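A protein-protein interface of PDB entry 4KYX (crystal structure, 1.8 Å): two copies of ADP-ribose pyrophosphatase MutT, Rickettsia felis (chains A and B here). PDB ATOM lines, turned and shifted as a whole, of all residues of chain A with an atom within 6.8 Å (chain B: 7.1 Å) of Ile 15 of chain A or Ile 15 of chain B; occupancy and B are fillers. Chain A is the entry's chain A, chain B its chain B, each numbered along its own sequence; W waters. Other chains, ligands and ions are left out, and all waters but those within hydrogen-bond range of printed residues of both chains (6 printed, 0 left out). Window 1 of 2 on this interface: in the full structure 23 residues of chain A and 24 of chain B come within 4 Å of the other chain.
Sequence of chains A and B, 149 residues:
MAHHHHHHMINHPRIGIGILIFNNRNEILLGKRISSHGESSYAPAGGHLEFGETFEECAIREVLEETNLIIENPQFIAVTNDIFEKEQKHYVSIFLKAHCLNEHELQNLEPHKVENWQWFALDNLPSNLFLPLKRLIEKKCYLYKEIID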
ATOM      1  N   HIS A  12     -29.181  25.700  31.780  1.00  0.00           N
ATOM      2  CA  HIS A  12     -27.740  25.642  31.573  1.00  0.00           C
ATOM      3  C   HIS A  12     -27.331  25.682  30.072  1.00  0.00           C
ATOM      4  O   HIS A  12     -27.997  25.095  29.212  1.00  0.00           O
ATOM      5  CB  HIS A  12     -27.207  24.342  32.189  1.00  0.00           C
ATOM      6  CG  HIS A  12     -27.409  24.248  33.671  1.00  0.00           C
ATOM      7  ND1 HIS A  12     -27.666  23.057  34.315  1.00  0.00           N
ATOM      8  CD2 HIS A  12     -27.394  25.201  34.635  1.00  0.00           C
ATOM      9  CE1 HIS A  12     -27.777  23.275  35.612  1.00  0.00           C
ATOM     10  NE2 HIS A  12     -27.610  24.570  35.836  1.00  0.00           N
ATOM     11  N   PRO A  13     -26.193  26.332  29.769  1.00  0.00           N
ATOM     12  CA  PRO A  13     -25.565  26.196  28.458  1.00  0.00           C
ATOM     13  C   PRO A  13     -25.364  24.712  28.057  1.00  0.00           C
ATOM     14  O   PRO A  13     -24.968  23.889  28.883  1.00  0.00           O
ATOM     15  CB  PRO A  13     -24.201  26.892  28.671  1.00  0.00           C
ATOM     16  CG  PRO A  13     -24.452  27.860  29.755  1.00  0.00           C
ATOM     17  CD  PRO A  13     -25.371  27.151  30.689  1.00  0.00           C
ATOM     18  N   ARG A  14     -25.631  24.401  26.801  1.00  0.00           N
ATOM     19  CA  ARG A  14     -25.504  23.035  26.317  1.00  0.00           C
ATOM     20  C   ARG A  14     -24.403  22.875  25.303  1.00  0.00           C
ATOM     21  O   ARG A  14     -24.063  23.805  24.637  1.00  0.00           O
ATOM     22  CB  ARG A  14     -26.835  22.636  25.705  1.00  0.00           C
ATOM     23  CG  ARG A  14     -28.011  22.698  26.666  1.00  0.00           C
ATOM     24  CD  ARG A  14     -28.207  21.414  27.483  1.00  0.00           C
ATOM     25  NE  ARG A  14     -27.721  20.170  26.854  1.00  0.00           N
ATOM     26  CZ  ARG A  14     -28.439  19.243  26.223  1.00  0.00           C
ATOM     27  NH1 ARG A  14     -29.758  19.361  26.019  1.00  0.00           N
ATOM     28  NH2 ARG A  14     -27.805  18.170  25.764  1.00  0.00           N
ATOM     29  N   ILE A  15     -23.901  21.662  25.100  1.00  0.00           N
ATOM     30  CA  ILE A  15     -22.843  21.478  24.176  1.00  0.00           C
ATOM     31  C   ILE A  15     -23.380  20.746  22.942  1.00  0.00           C
ATOM     32  O   ILE A  15     -23.945  19.666  23.038  1.00  0.00           O
ATOM     33  CB  ILE A  15     -21.686  20.681  24.774  1.00  0.00           C
ATOM     34  CG1 ILE A  15     -21.077  21.449  25.960  1.00  0.00           C
ATOM     35  CG2 ILE A  15     -20.693  20.366  23.670  1.00  0.00           C
ATOM     36  CD1 ILE A  15     -20.588  20.614  27.122  1.00  0.00           C
ATOM     37  N   GLY A  16     -23.136  21.351  21.797  1.00  0.00           N
ATOM     38  CA  GLY A  16     -23.562  20.844  20.504  1.00  0.00           C
ATOM     39  C   GLY A  16     -22.314  20.468  19.726  1.00  0.00           C
ATOM     40  O   GLY A  16     -21.261  21.095  19.843  1.00  0.00           O
ATOM     41  N   ILE A  17     -22.423  19.470  18.868  1.00  0.00           N
ATOM     42  CA  ILE A  17     -21.353  19.091  17.982  1.00  0.00           C
ATOM     43  C   ILE A  17     -21.864  19.388  16.562  1.00  0.00           C
ATOM     44  O   ILE A  17     -22.931  18.886  16.175  1.00  0.00           O
ATOM     45  CB  ILE A  17     -21.025  17.574  18.154  1.00  0.00           C
ATOM     46  CG1 ILE A  17     -20.465  17.203  19.536  1.00  0.00           C
ATOM     47  CG2 ILE A  17     -20.192  17.061  16.988  1.00  0.00           C
ATOM     48  CD1 ILE A  17     -19.351  18.024  20.076  1.00  0.00           C
ATOM     49  N   GLY A  47     -25.605  17.563  16.530  1.00  0.00           N
ATOM     50  CA  GLY A  47     -26.593  17.513  17.544  1.00  0.00           C
ATOM     51  C   GLY A  47     -25.858  17.512  18.866  1.00  0.00           C
ATOM     52  O   GLY A  47     -24.711  17.978  18.944  1.00  0.00           O
ATOM     53  N   HIS A  48     -26.495  16.958  19.878  1.00  0.00           N
ATOM     54  CA  HIS A  48     -26.016  17.161  21.240  1.00  0.00           C
ATOM     55  C   HIS A  48     -24.920  16.172  21.608  1.00  0.00           C
ATOM     56  O   HIS A  48     -25.022  14.978  21.305  1.00  0.00           O
ATOM     57  CB  HIS A  48     -27.163  16.926  22.188  1.00  0.00           C
ATOM     58  CG  HIS A  48     -28.141  18.036  22.217  1.00  0.00           C
ATOM     59  ND1 HIS A  48     -29.488  17.835  22.031  1.00  0.00           N
ATOM     60  CD2 HIS A  48     -27.986  19.364  22.440  1.00  0.00           C
ATOM     61  CE1 HIS A  48     -30.127  18.990  22.104  1.00  0.00           C
ATOM     62  NE2 HIS A  48     -29.242  19.935  22.354  1.00  0.00           N
ATOM     63  N   LEU A  49     -23.879  16.647  22.289  1.00  0.00           N
ATOM     64  CA  LEU A  49     -22.893  15.738  22.885  1.00  0.00           C
ATOM     65  C   LEU A  49     -23.595  14.926  23.981  1.00  0.00           C
ATOM     66  O   LEU A  49     -24.296  15.486  24.820  1.00  0.00           O
ATOM     67  CB  LEU A  49     -21.731  16.548  23.502  1.00  0.00           C
ATOM     68  CG  LEU A  49     -20.590  15.709  24.094  1.00  0.00           C
ATOM     69  CD1 LEU A  49     -19.839  14.896  23.049  1.00  0.00           C
ATOM     70  CD2 LEU A  49     -19.635  16.649  24.772  1.00  0.00           C
ATOM     71  N   GLU A  50     -23.442  13.614  23.962  1.00  0.00           N
ATOM     72  CA  GLU A  50     -24.051  12.795  24.984  1.00  0.00           C
ATOM     73  C   GLU A  50     -23.043  12.506  26.081  1.00  0.00           C
ATOM     74  O   GLU A  50     -21.820  12.534  25.872  1.00  0.00           O
ATOM     75  CB  GLU A  50     -24.588  11.477  24.427  1.00  0.00           C
ATOM     76  CG  GLU A  50     -25.788  11.650  23.517  1.00  0.00           C
ATOM     77  CD  GLU A  50     -26.291  10.338  22.917  1.00  0.00           C
ATOM     78  OE1 GLU A  50     -25.825   9.258  23.326  1.00  0.00           O
ATOM     79  OE2 GLU A  50     -27.145  10.416  21.989  1.00  0.00           O
ATOM     80  N   PHE A  55     -15.675  14.065  21.511  1.00  0.00           N
ATOM     81  CA  PHE A  55     -16.196  14.911  20.429  1.00  0.00           C
ATOM     82  C   PHE A  55     -16.144  14.102  19.155  1.00  0.00           C
ATOM     83  O   PHE A  55     -17.066  14.210  18.385  1.00  0.00           O
ATOM     84  CB  PHE A  55     -15.395  16.172  20.195  1.00  0.00           C
ATOM     85  CG  PHE A  55     -15.317  17.111  21.405  1.00  0.00           C
ATOM     86  CD1 PHE A  55     -16.310  17.125  22.372  1.00  0.00           C
ATOM     87  CD2 PHE A  55     -14.217  17.948  21.562  1.00  0.00           C
ATOM     88  CE1 PHE A  55     -16.197  17.963  23.477  1.00  0.00           C
ATOM     89  CE2 PHE A  55     -14.113  18.799  22.640  1.00  0.00           C
ATOM     90  CZ  PHE A  55     -15.097  18.807  23.592  1.00  0.00           C
ATOM     91  N   ASN A  81     -19.972  30.205  20.577  1.00  0.00           N
ATOM     92  CA  ASN A  81     -20.770  30.384  21.767  1.00  0.00           C
ATOM     93  C   ASN A  81     -21.961  31.263  21.404  1.00  0.00           C
ATOM     94  O   ASN A  81     -21.802  32.448  21.167  1.00  0.00           O
ATOM     95  CB  ASN A  81     -19.895  31.054  22.845  1.00  0.00           C
ATOM     96  CG  ASN A  81     -20.676  31.437  24.083  1.00  0.00           C
ATOM     97  OD1 ASN A  81     -21.433  30.655  24.602  1.00  0.00           O
ATOM     98  ND2 ASN A  81     -20.518  32.655  24.530  1.00  0.00           N
ATOM     99  N   HIS A  90     -28.937  28.375  25.047  1.00  0.00           N
ATOM    100  CA  HIS A  90     -27.565  28.828  24.932  1.00  0.00           C
ATOM    101  C   HIS A  90     -26.740  27.560  24.588  1.00  0.00           C
ATOM    102  O   HIS A  90     -26.743  26.609  25.365  1.00  0.00           O
ATOM    103  CB  HIS A  90     -27.159  29.401  26.287  1.00  0.00           C
ATOM    104  CG  HIS A  90     -25.741  29.877  26.363  1.00  0.00           C
ATOM    105  ND1 HIS A  90     -25.299  30.681  27.383  1.00  0.00           N
ATOM    106  CD2 HIS A  90     -24.672  29.689  25.548  1.00  0.00           C
ATOM    107  CE1 HIS A  90     -24.024  30.962  27.214  1.00  0.00           C
ATOM    108  NE2 HIS A  90     -23.611  30.364  26.120  1.00  0.00           N
ATOM    109  N   TYR A  91     -26.049  27.570  23.450  1.00  0.00           N
ATOM    110  CA  TYR A  91     -25.240  26.461  22.998  1.00  0.00           C
ATOM    111  C   TYR A  91     -23.819  26.848  22.769  1.00  0.00           C
ATOM    112  O   TYR A  91     -23.528  27.876  22.166  1.00  0.00           O
ATOM    113  CB  TYR A  91     -25.755  25.938  21.660  1.00  0.00           C
ATOM    114  CG  TYR A  91     -26.904  25.063  21.842  1.00  0.00           C
ATOM    115  CD1 TYR A  91     -26.726  23.725  22.107  1.00  0.00           C
ATOM    116  CD2 TYR A  91     -28.211  25.564  21.752  1.00  0.00           C
ATOM    117  CE1 TYR A  91     -27.813  22.885  22.271  1.00  0.00           C
ATOM    118  CE2 TYR A  91     -29.309  24.729  21.936  1.00  0.00           C
ATOM    119  CZ  TYR A  91     -29.096  23.395  22.202  1.00  0.00           C
ATOM    120  OH  TYR A  91     -30.159  22.542  22.365  1.00  0.00           O
ATOM    121  N   VAL A  92     -22.921  26.012  23.255  1.00  0.00           N
ATOM    122  CA  VAL A  92     -21.552  26.066  22.834  1.00  0.00           C
ATOM    123  C   VAL A  92     -21.426  24.996  21.770  1.00  0.00           C
ATOM    124  O   VAL A  92     -21.641  23.806  22.046  1.00  0.00           O
ATOM    125  CB  VAL A  92     -20.594  25.872  24.025  1.00  0.00           C
ATOM    126  CG1 VAL A  92     -19.170  25.662  23.565  1.00  0.00           C
ATOM    127  CG2 VAL A  92     -20.667  27.094  24.956  1.00  0.00           C
ATOM    128  N   SER A  93     -21.132  25.398  20.530  1.00  0.00           N
ATOM    129  CA  SER A  93     -20.980  24.430  19.452  1.00  0.00           C
ATOM    130  C   SER A  93     -19.509  24.105  19.214  1.00  0.00           C
ATOM    131  O   SER A  93     -18.675  24.997  19.099  1.00  0.00           O
ATOM    132  CB  SER A  93     -21.574  24.942  18.161  1.00  0.00           C
ATOM    133  OG  SER A  93     -22.984  25.171  18.307  1.00  0.00           O
ATOM    134  N   ILE A  94     -19.213  22.834  19.081  1.00  0.00           N
ATOM    135  CA  ILE A  94     -17.904  22.364  18.693  1.00  0.00           C
ATOM    136  C   ILE A  94     -18.005  21.860  17.284  1.00  0.00           C
ATOM    137  O   ILE A  94     -18.807  20.967  17.002  1.00  0.00           O
ATOM    138  CB  ILE A  94     -17.490  21.179  19.565  1.00  0.00           C
ATOM    139  CG1 ILE A  94     -17.604  21.568  21.031  1.00  0.00           C
ATOM    140  CG2 ILE A  94     -16.108  20.679  19.177  1.00  0.00           C
ATOM    141  CD1 ILE A  94     -16.681  22.624  21.471  1.00  0.00           C
ATOM    142  N   HIS B  12     -26.698  15.803  31.176  1.00  0.00           N
ATOM    143  CA  HIS B  12     -26.072  16.469  30.060  1.00  0.00           C
ATOM    144  C   HIS B  12     -24.632  16.835  30.431  1.00  0.00           C
ATOM    145  O   HIS B  12     -24.370  17.224  31.585  1.00  0.00           O
ATOM    146  CB  HIS B  12     -26.823  17.737  29.732  1.00  0.00           C
ATOM    147  CG  HIS B  12     -28.257  17.530  29.344  1.00  0.00           C
ATOM    148  ND1 HIS B  12     -28.716  16.403  28.706  1.00  0.00           N
ATOM    149  CD2 HIS B  12     -29.321  18.359  29.452  1.00  0.00           C
ATOM    150  CE1 HIS B  12     -30.007  16.539  28.447  1.00  0.00           C
ATOM    151  NE2 HIS B  12     -30.398  17.715  28.906  1.00  0.00           N
ATOM    152  N   PRO B  13     -23.692  16.704  29.493  1.00  0.00           N
ATOM    153  CA  PRO B  13     -22.368  17.374  29.679  1.00  0.00           C
ATOM    154  C   PRO B  13     -22.545  18.880  30.005  1.00  0.00           C
ATOM    155  O   PRO B  13     -23.399  19.569  29.438  1.00  0.00           O
ATOM    156  CB  PRO B  13     -21.695  17.220  28.308  1.00  0.00           C
ATOM    157  CG  PRO B  13     -22.381  16.011  27.733  1.00  0.00           C
ATOM    158  CD  PRO B  13     -23.801  16.123  28.164  1.00  0.00           C
ATOM    159  N   ARG B  14     -21.750  19.344  30.927  1.00  0.00           N
ATOM    160  CA  ARG B  14     -21.830  20.685  31.399  1.00  0.00           C
ATOM    161  C   ARG B  14     -20.614  21.461  30.937  1.00  0.00           C
ATOM    162  O   ARG B  14     -19.542  20.888  30.771  1.00  0.00           O
ATOM    163  CB  ARG B  14     -21.849  20.674  32.930  1.00  0.00           C
ATOM    164  CG  ARG B  14     -23.105  20.080  33.556  1.00  0.00           C
ATOM    165  CD  ARG B  14     -24.354  20.928  33.293  1.00  0.00           C
ATOM    166  NE  ARG B  14     -24.180  22.364  33.562  1.00  0.00           N
ATOM    167  CZ  ARG B  14     -24.268  22.960  34.755  1.00  0.00           C
ATOM    168  NH1 ARG B  14     -24.506  22.255  35.871  1.00  0.00           N
ATOM    169  NH2 ARG B  14     -24.093  24.285  34.842  1.00  0.00           N
ATOM    170  N   ILE B  15     -20.726  22.789  30.898  1.00  0.00           N
ATOM    171  CA  ILE B  15     -19.622  23.611  30.462  1.00  0.00           C
ATOM    172  C   ILE B  15     -19.004  24.287  31.679  1.00  0.00           C
ATOM    173  O   ILE B  15     -19.702  25.024  32.380  1.00  0.00           O
ATOM    174  CB  ILE B  15     -20.054  24.687  29.470  1.00  0.00           C
ATOM    175  CG1 ILE B  15     -20.582  23.997  28.185  1.00  0.00           C
ATOM    176  CG2 ILE B  15     -18.891  25.597  29.149  1.00  0.00           C
ATOM    177  CD1 ILE B  15     -21.617  24.746  27.457  1.00  0.00           C
ATOM    178  N   GLY B  16     -17.701  24.083  31.858  1.00  0.00           N
ATOM    179  CA  GLY B  16     -16.897  24.842  32.840  1.00  0.00           C
ATOM    180  C   GLY B  16     -15.902  25.775  32.213  1.00  0.00           C
ATOM    181  O   GLY B  16     -15.471  25.569  31.100  1.00  0.00           O
ATOM    182  N   ILE B  17     -15.620  26.864  32.917  1.00  0.00           N
ATOM    183  CA  ILE B  17     -14.636  27.867  32.556  1.00  0.00           C
ATOM    184  C   ILE B  17     -13.475  27.729  33.546  1.00  0.00           C
ATOM    185  O   ILE B  17     -13.694  27.645  34.747  1.00  0.00           O
ATOM    186  CB  ILE B  17     -15.266  29.273  32.641  1.00  0.00           C
ATOM    187  CG1 ILE B  17     -16.444  29.418  31.655  1.00  0.00           C
ATOM    188  CG2 ILE B  17     -14.211  30.364  32.551  1.00  0.00           C
ATOM    189  CD1 ILE B  17     -16.195  29.157  30.207  1.00  0.00           C
ATOM    190  N   GLY B  47     -15.432  28.067  37.175  1.00  0.00           N
ATOM    191  CA  GLY B  47     -16.711  27.619  37.673  1.00  0.00           C
ATOM    192  C   GLY B  47     -17.575  27.451  36.439  1.00  0.00           C
ATOM    193  O   GLY B  47     -17.055  27.429  35.309  1.00  0.00           O
ATOM    194  N   HIS B  48     -18.872  27.357  36.636  1.00  0.00           N
ATOM    195  CA  HIS B  48     -19.788  27.080  35.534  1.00  0.00           C
ATOM    196  C   HIS B  48     -20.069  28.288  34.647  1.00  0.00           C
ATOM    197  O   HIS B  48     -20.289  29.341  35.120  1.00  0.00           O
ATOM    198  CB  HIS B  48     -21.143  26.630  36.117  1.00  0.00           C
ATOM    199  CG  HIS B  48     -21.104  25.278  36.743  1.00  0.00           C
ATOM    200  ND1 HIS B  48     -21.663  25.008  37.973  1.00  0.00           N
ATOM    201  CD2 HIS B  48     -20.554  24.118  36.313  1.00  0.00           C
ATOM    202  CE1 HIS B  48     -21.479  23.734  38.271  1.00  0.00           C
ATOM    203  NE2 HIS B  48     -20.814  23.170  37.278  1.00  0.00           N
ATOM    204  N   LEU B  49     -20.165  28.094  33.345  1.00  0.00           N
ATOM    205  CA  LEU B  49     -20.645  29.157  32.465  1.00  0.00           C
ATOM    206  C   LEU B  49     -22.130  29.348  32.718  1.00  0.00           C
ATOM    207  O   LEU B  49     -22.898  28.382  32.671  1.00  0.00           O
ATOM    208  CB  LEU B  49     -20.430  28.754  31.003  1.00  0.00           C
ATOM    209  CG  LEU B  49     -20.810  29.743  29.901  1.00  0.00           C
ATOM    210  CD1 LEU B  49     -19.939  30.995  29.944  1.00  0.00           C
ATOM    211  CD2 LEU B  49     -20.655  29.088  28.566  1.00  0.00           C
ATOM    212  N   GLU B  50     -22.559  30.584  32.915  1.00  0.00           N
ATOM    213  CA  GLU B  50     -23.944  30.889  33.189  1.00  0.00           C
ATOM    214  C   GLU B  50     -24.624  31.238  31.869  1.00  0.00           C
ATOM    215  O   GLU B  50     -23.960  31.719  30.922  1.00  0.00           O
ATOM    216  CB  GLU B  50     -24.056  32.028  34.213  1.00  0.00           C
ATOM    217  CG  GLU B  50     -23.642  31.536  35.610  1.00  0.00           C
ATOM    218  CD  GLU B  50     -23.594  32.615  36.668  1.00  0.00           C
ATOM    219  OE1 GLU B  50     -23.898  33.793  36.352  1.00  0.00           O
ATOM    220  OE2 GLU B  50     -23.222  32.275  37.823  1.00  0.00           O
ATOM    221  N   PHE B  55     -17.523  33.632  27.001  1.00  0.00           N
ATOM    222  CA  PHE B  55     -16.454  33.000  27.774  1.00  0.00           C
ATOM    223  C   PHE B  55     -15.645  34.067  28.564  1.00  0.00           C
ATOM    224  O   PHE B  55     -15.260  33.856  29.676  1.00  0.00           O
ATOM    225  CB  PHE B  55     -15.463  32.176  26.916  1.00  0.00           C
ATOM    226  CG  PHE B  55     -16.086  31.037  26.135  1.00  0.00           C
ATOM    227  CD1 PHE B  55     -17.227  30.412  26.568  1.00  0.00           C
ATOM    228  CD2 PHE B  55     -15.473  30.587  24.995  1.00  0.00           C
ATOM    229  CE1 PHE B  55     -17.759  29.346  25.856  1.00  0.00           C
ATOM    230  CE2 PHE B  55     -15.982  29.547  24.304  1.00  0.00           C
ATOM    231  CZ  PHE B  55     -17.128  28.919  24.729  1.00  0.00           C
ATOM    232  N   ASN B  81     -12.048  17.816  27.483  1.00  0.00           N
ATOM    233  CA  ASN B  81     -13.234  16.987  27.570  1.00  0.00           C
ATOM    234  C   ASN B  81     -13.043  15.957  28.666  1.00  0.00           C
ATOM    235  O   ASN B  81     -12.254  15.045  28.520  1.00  0.00           O
ATOM    236  CB  ASN B  81     -13.527  16.328  26.220  1.00  0.00           C
ATOM    237  CG  ASN B  81     -14.863  15.651  26.212  1.00  0.00           C
ATOM    238  OD1 ASN B  81     -15.828  16.170  26.696  1.00  0.00           O
ATOM    239  ND2 ASN B  81     -14.909  14.480  25.681  1.00  0.00           N
ATOM    240  N   HIS B  90     -19.867  14.930  33.499  1.00  0.00           N
ATOM    241  CA  HIS B  90     -19.121  15.100  32.280  1.00  0.00           C
ATOM    242  C   HIS B  90     -19.005  16.602  32.067  1.00  0.00           C
ATOM    243  O   HIS B  90     -20.011  17.261  31.890  1.00  0.00           O
ATOM    244  CB  HIS B  90     -19.900  14.458  31.112  1.00  0.00           C
ATOM    245  CG  HIS B  90     -19.183  14.479  29.807  1.00  0.00           C
ATOM    246  ND1 HIS B  90     -19.571  13.694  28.745  1.00  0.00           N
ATOM    247  CD2 HIS B  90     -18.120  15.199  29.369  1.00  0.00           C
ATOM    248  CE1 HIS B  90     -18.807  13.938  27.699  1.00  0.00           C
ATOM    249  NE2 HIS B  90     -17.898  14.827  28.054  1.00  0.00           N
ATOM    250  N   TYR B  91     -17.779  17.090  32.008  1.00  0.00           N
ATOM    251  CA  TYR B  91     -17.513  18.496  31.807  1.00  0.00           C
ATOM    252  C   TYR B  91     -16.687  18.731  30.559  1.00  0.00           C
ATOM    253  O   TYR B  91     -15.665  18.103  30.349  1.00  0.00           O
ATOM    254  CB  TYR B  91     -16.776  19.142  32.982  1.00  0.00           C
ATOM    255  CG  TYR B  91     -17.696  19.601  34.042  1.00  0.00           C
ATOM    256  CD1 TYR B  91     -18.284  20.849  33.974  1.00  0.00           C
ATOM    257  CD2 TYR B  91     -18.024  18.766  35.106  1.00  0.00           C
ATOM    258  CE1 TYR B  91     -19.154  21.289  34.966  1.00  0.00           C
ATOM    259  CE2 TYR B  91     -18.907  19.170  36.093  1.00  0.00           C
ATOM    260  CZ  TYR B  91     -19.473  20.423  36.017  1.00  0.00           C
ATOM    261  OH  TYR B  91     -20.339  20.827  37.002  1.00  0.00           O
ATOM    262  N   VAL B  92     -17.098  19.736  29.820  1.00  0.00           N
ATOM    263  CA  VAL B  92     -16.274  20.329  28.786  1.00  0.00           C
ATOM    264  C   VAL B  92     -15.708  21.610  29.368  1.00  0.00           C
ATOM    265  O   VAL B  92     -16.461  22.480  29.800  1.00  0.00           O
ATOM    266  CB  VAL B  92     -17.051  20.559  27.500  1.00  0.00           C
ATOM    267  CG1 VAL B  92     -16.246  21.328  26.479  1.00  0.00           C
ATOM    268  CG2 VAL B  92     -17.457  19.198  26.956  1.00  0.00           C
ATOM    269  N   SER B  93     -14.382  21.690  29.458  1.00  0.00           N
ATOM    270  CA  SER B  93     -13.782  22.863  30.094  1.00  0.00           C
ATOM    271  C   SER B  93     -13.209  23.774  29.062  1.00  0.00           C
ATOM    272  O   SER B  93     -12.538  23.318  28.139  1.00  0.00           O
ATOM    273  CB  SER B  93     -12.678  22.477  31.058  1.00  0.00           C
ATOM    274  OG  SER B  93     -13.244  21.832  32.201  1.00  0.00           O
ATOM    275  N   ILE B  94     -13.526  25.060  29.191  1.00  0.00           N
ATOM    276  CA  ILE B  94     -12.954  26.065  28.382  1.00  0.00           C
ATOM    277  C   ILE B  94     -11.921  26.853  29.204  1.00  0.00           C
ATOM    278  O   ILE B  94     -12.285  27.419  30.247  1.00  0.00           O
ATOM    279  CB  ILE B  94     -14.052  27.057  27.965  1.00  0.00           C
ATOM    280  CG1 ILE B  94     -15.227  26.322  27.302  1.00  0.00           C
ATOM    281  CG2 ILE B  94     -13.435  28.148  27.131  1.00  0.00           C
ATOM    282  CD1 ILE B  94     -14.923  25.724  25.967  1.00  0.00           C
HETATM  283  O   HOH W   1     -25.585  21.504  29.916  1.00  0.00           O
HETATM  284  O   HOH W   2     -13.213  14.798  22.893  1.00  0.00           O
HETATM  285  O   HOH W   3     -26.832  15.487  26.344  1.00  0.00           O
HETATM  286  O   HOH W   4     -17.567  33.533  24.147  1.00  0.00           O
HETATM  287  O   HOH W   5     -23.254  23.665  31.039  1.00  0.00           O
HETATM  288  O   HOH W   6     -24.492  19.771  27.063  1.00  0.00           O
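Of chain B, only Pro 13, Arg 14, Ile 15 and Val 92 come within 4 Å of Ile 15 of chain A. Ile 15 of chain B touches just these residues of chain A: Pro 13, Arg 14, Ile 15 and Val 92. Printed residues of chain A within 4 Å of Leu 49 of chain B: Pro 13 (3.3 Å). Of the printed residues of chain A, His 12 of chain B touches Arg 14. Of the printed residues of chain B, Pro 13 of chain A touches Ile 15, Leu 49 and Glu 50. Printed residues of chain B within 4 Å of Leu 49 of chain A: Pro 13. Ser 93 of chain A touches none of the printed residues of chain B. The nearest residue of chain B that does not touch Ile 15 of chain A is Tyr 91 of chain B (5.5 Å). The nearest residue of chain A that does not touch Ile 15 of chain B is Tyr 91 of chain A (5.6 Å).
Among the printed residues, merely in contact across the chains: His 12 of chain A with Arg 14 of chain B (3.4 Å), Pro 13 of chain A with Ile 15 of chain B (3.6 Å), Pro 13 of chain A with Leu 49 of chain B (3.3 Å), Pro 13 of chain A with Glu 50 of chain B (3.99 Å), Arg 14 of chain A with Ile 15 of chain B (3.8 Å), Ile 15 of chain A with Pro 13 of chain B (3.8 Å), Ile 15 of chain A with Arg 14 of chain B (3.8 Å), Ile 15 of chain A with Ile 15 of chain B (3.4 Å), Ile 15 of chain A with Val 92 of chain B (3.4 Å), Leu 49 of chain A with Pro 13 of chain B (3.4 Å), Glu 50 of chain A with Pro 13 of chain B (3.9 Å), Glu 50 of chain A with His 90 of chain B (3.8 Å), Phe 55 of chain A with Asn 81 of chain B (3.7 Å), Phe 55 of chain A with Val 92 of chain B (3.9 Å), Asn 81 of chain A with Phe 55 of chain B (3.97 Å), His 90 of chain A with Glu 50 of chain B (3.8 Å), Val 92 of chain A with Ile 15 of chain B (3.6 Å) and Val 92 of chain A with Phe 55 of chain B (3.8 Å).
Pro 13 of chain A touches Ile 15 of chain B, and with the chains exchanged Ile 15 of chain A touches Pro 13 of chain B. Pro 13 of chain A touches Leu 49 of chain B, and with the chains exchanged Leu 49 of chain A touches Pro 13 of chain B. Pro 13 of chain A touches Glu 50 of chain B, and with the chains exchanged Glu 50 of chain A touches Pro 13 of chain B. Phe 55 of chain A touches Asn 81 of chain B, and with the chains exchanged Asn 81 of chain A touches Phe 55 of chain B. Positions printed for both chains: 12, 13, 14, 15, 16, 17, 47, 48, 49, 50, 55, 81, 90, 91, 92, 93 and 94. Of the 19 pairs that touch across the chains among the printed residues, 19 have their exchanged pair printed and touching as well.
The side-chain amide oxygen (OD1) of Asn 81 of chain A sits at hydrogen-bond distance from a ring nitrogen (NE2) of His 90 of chain A. The backbone NH (N) of Arg 14 of chain B lies within hydrogen-bond range of the backbone carbonyl oxygen (O) of His 90 of chain B, 2.9 Å away. The backbone carbonyl oxygen (O) of Arg 14 of chain B sits at hydrogen-bond distance from the backbone NH (N) of Val 92 of chain B, at 2.9 Å. N of Gly 16 of chain B lies within hydrogen-bond range of O of Val 92 of chain B, at 2.9 Å. The side-chain amide oxygen of Asn 81 of chain B is in hydrogen-bond range of a ring nitrogen (NE2) of His 90 of chain B (2.8 Å).
NH1 of Arg 14 of chain A sits at hydrogen-bond distance from NE2 of His 12 of chain B, 3.4 Å away.
Water W6 lies within hydrogen-bond range of the backbone carbonyl oxygen (O) of Pro 13 of chain B (2.6 Å), the backbone NH (N) of Ile 15 of chain A (2.8 Å) and the guanidinium group (NE) of Arg 14 of chain A (3.3 Å). Water W4 bridges the backbone NH of Phe 55 of chain B (2.9 Å) and the side-chain amide nitrogen of Asn 81 of chain A (3.1 Å). Water W3 lies within hydrogen-bond range of NH2 of Arg 14 of chain A (2.9 Å), O of Leu 49 of chain A (3.0 Å) and ND1 of His 12 of chain B (3.2 Å). Water W2 lies within hydrogen-bond range of the backbone NH (N) of Phe 55 of chain A and the side-chain amide nitrogen (ND2) of Asn 81 of chain B.
Of the 17 printed residues of chain A, 10 touch a printed residue of chain B. Hydrophobic or aromatic side chains of chain A within 4 Å of the printed part of chain B: His 12, Pro 13, Ile 15, Phe 55, His 90 and Val 92. Among the printed residues, no Asp or Glu carboxylate lies within 4 Å of a Lys or Arg side-chain nitrogen of the other chain.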
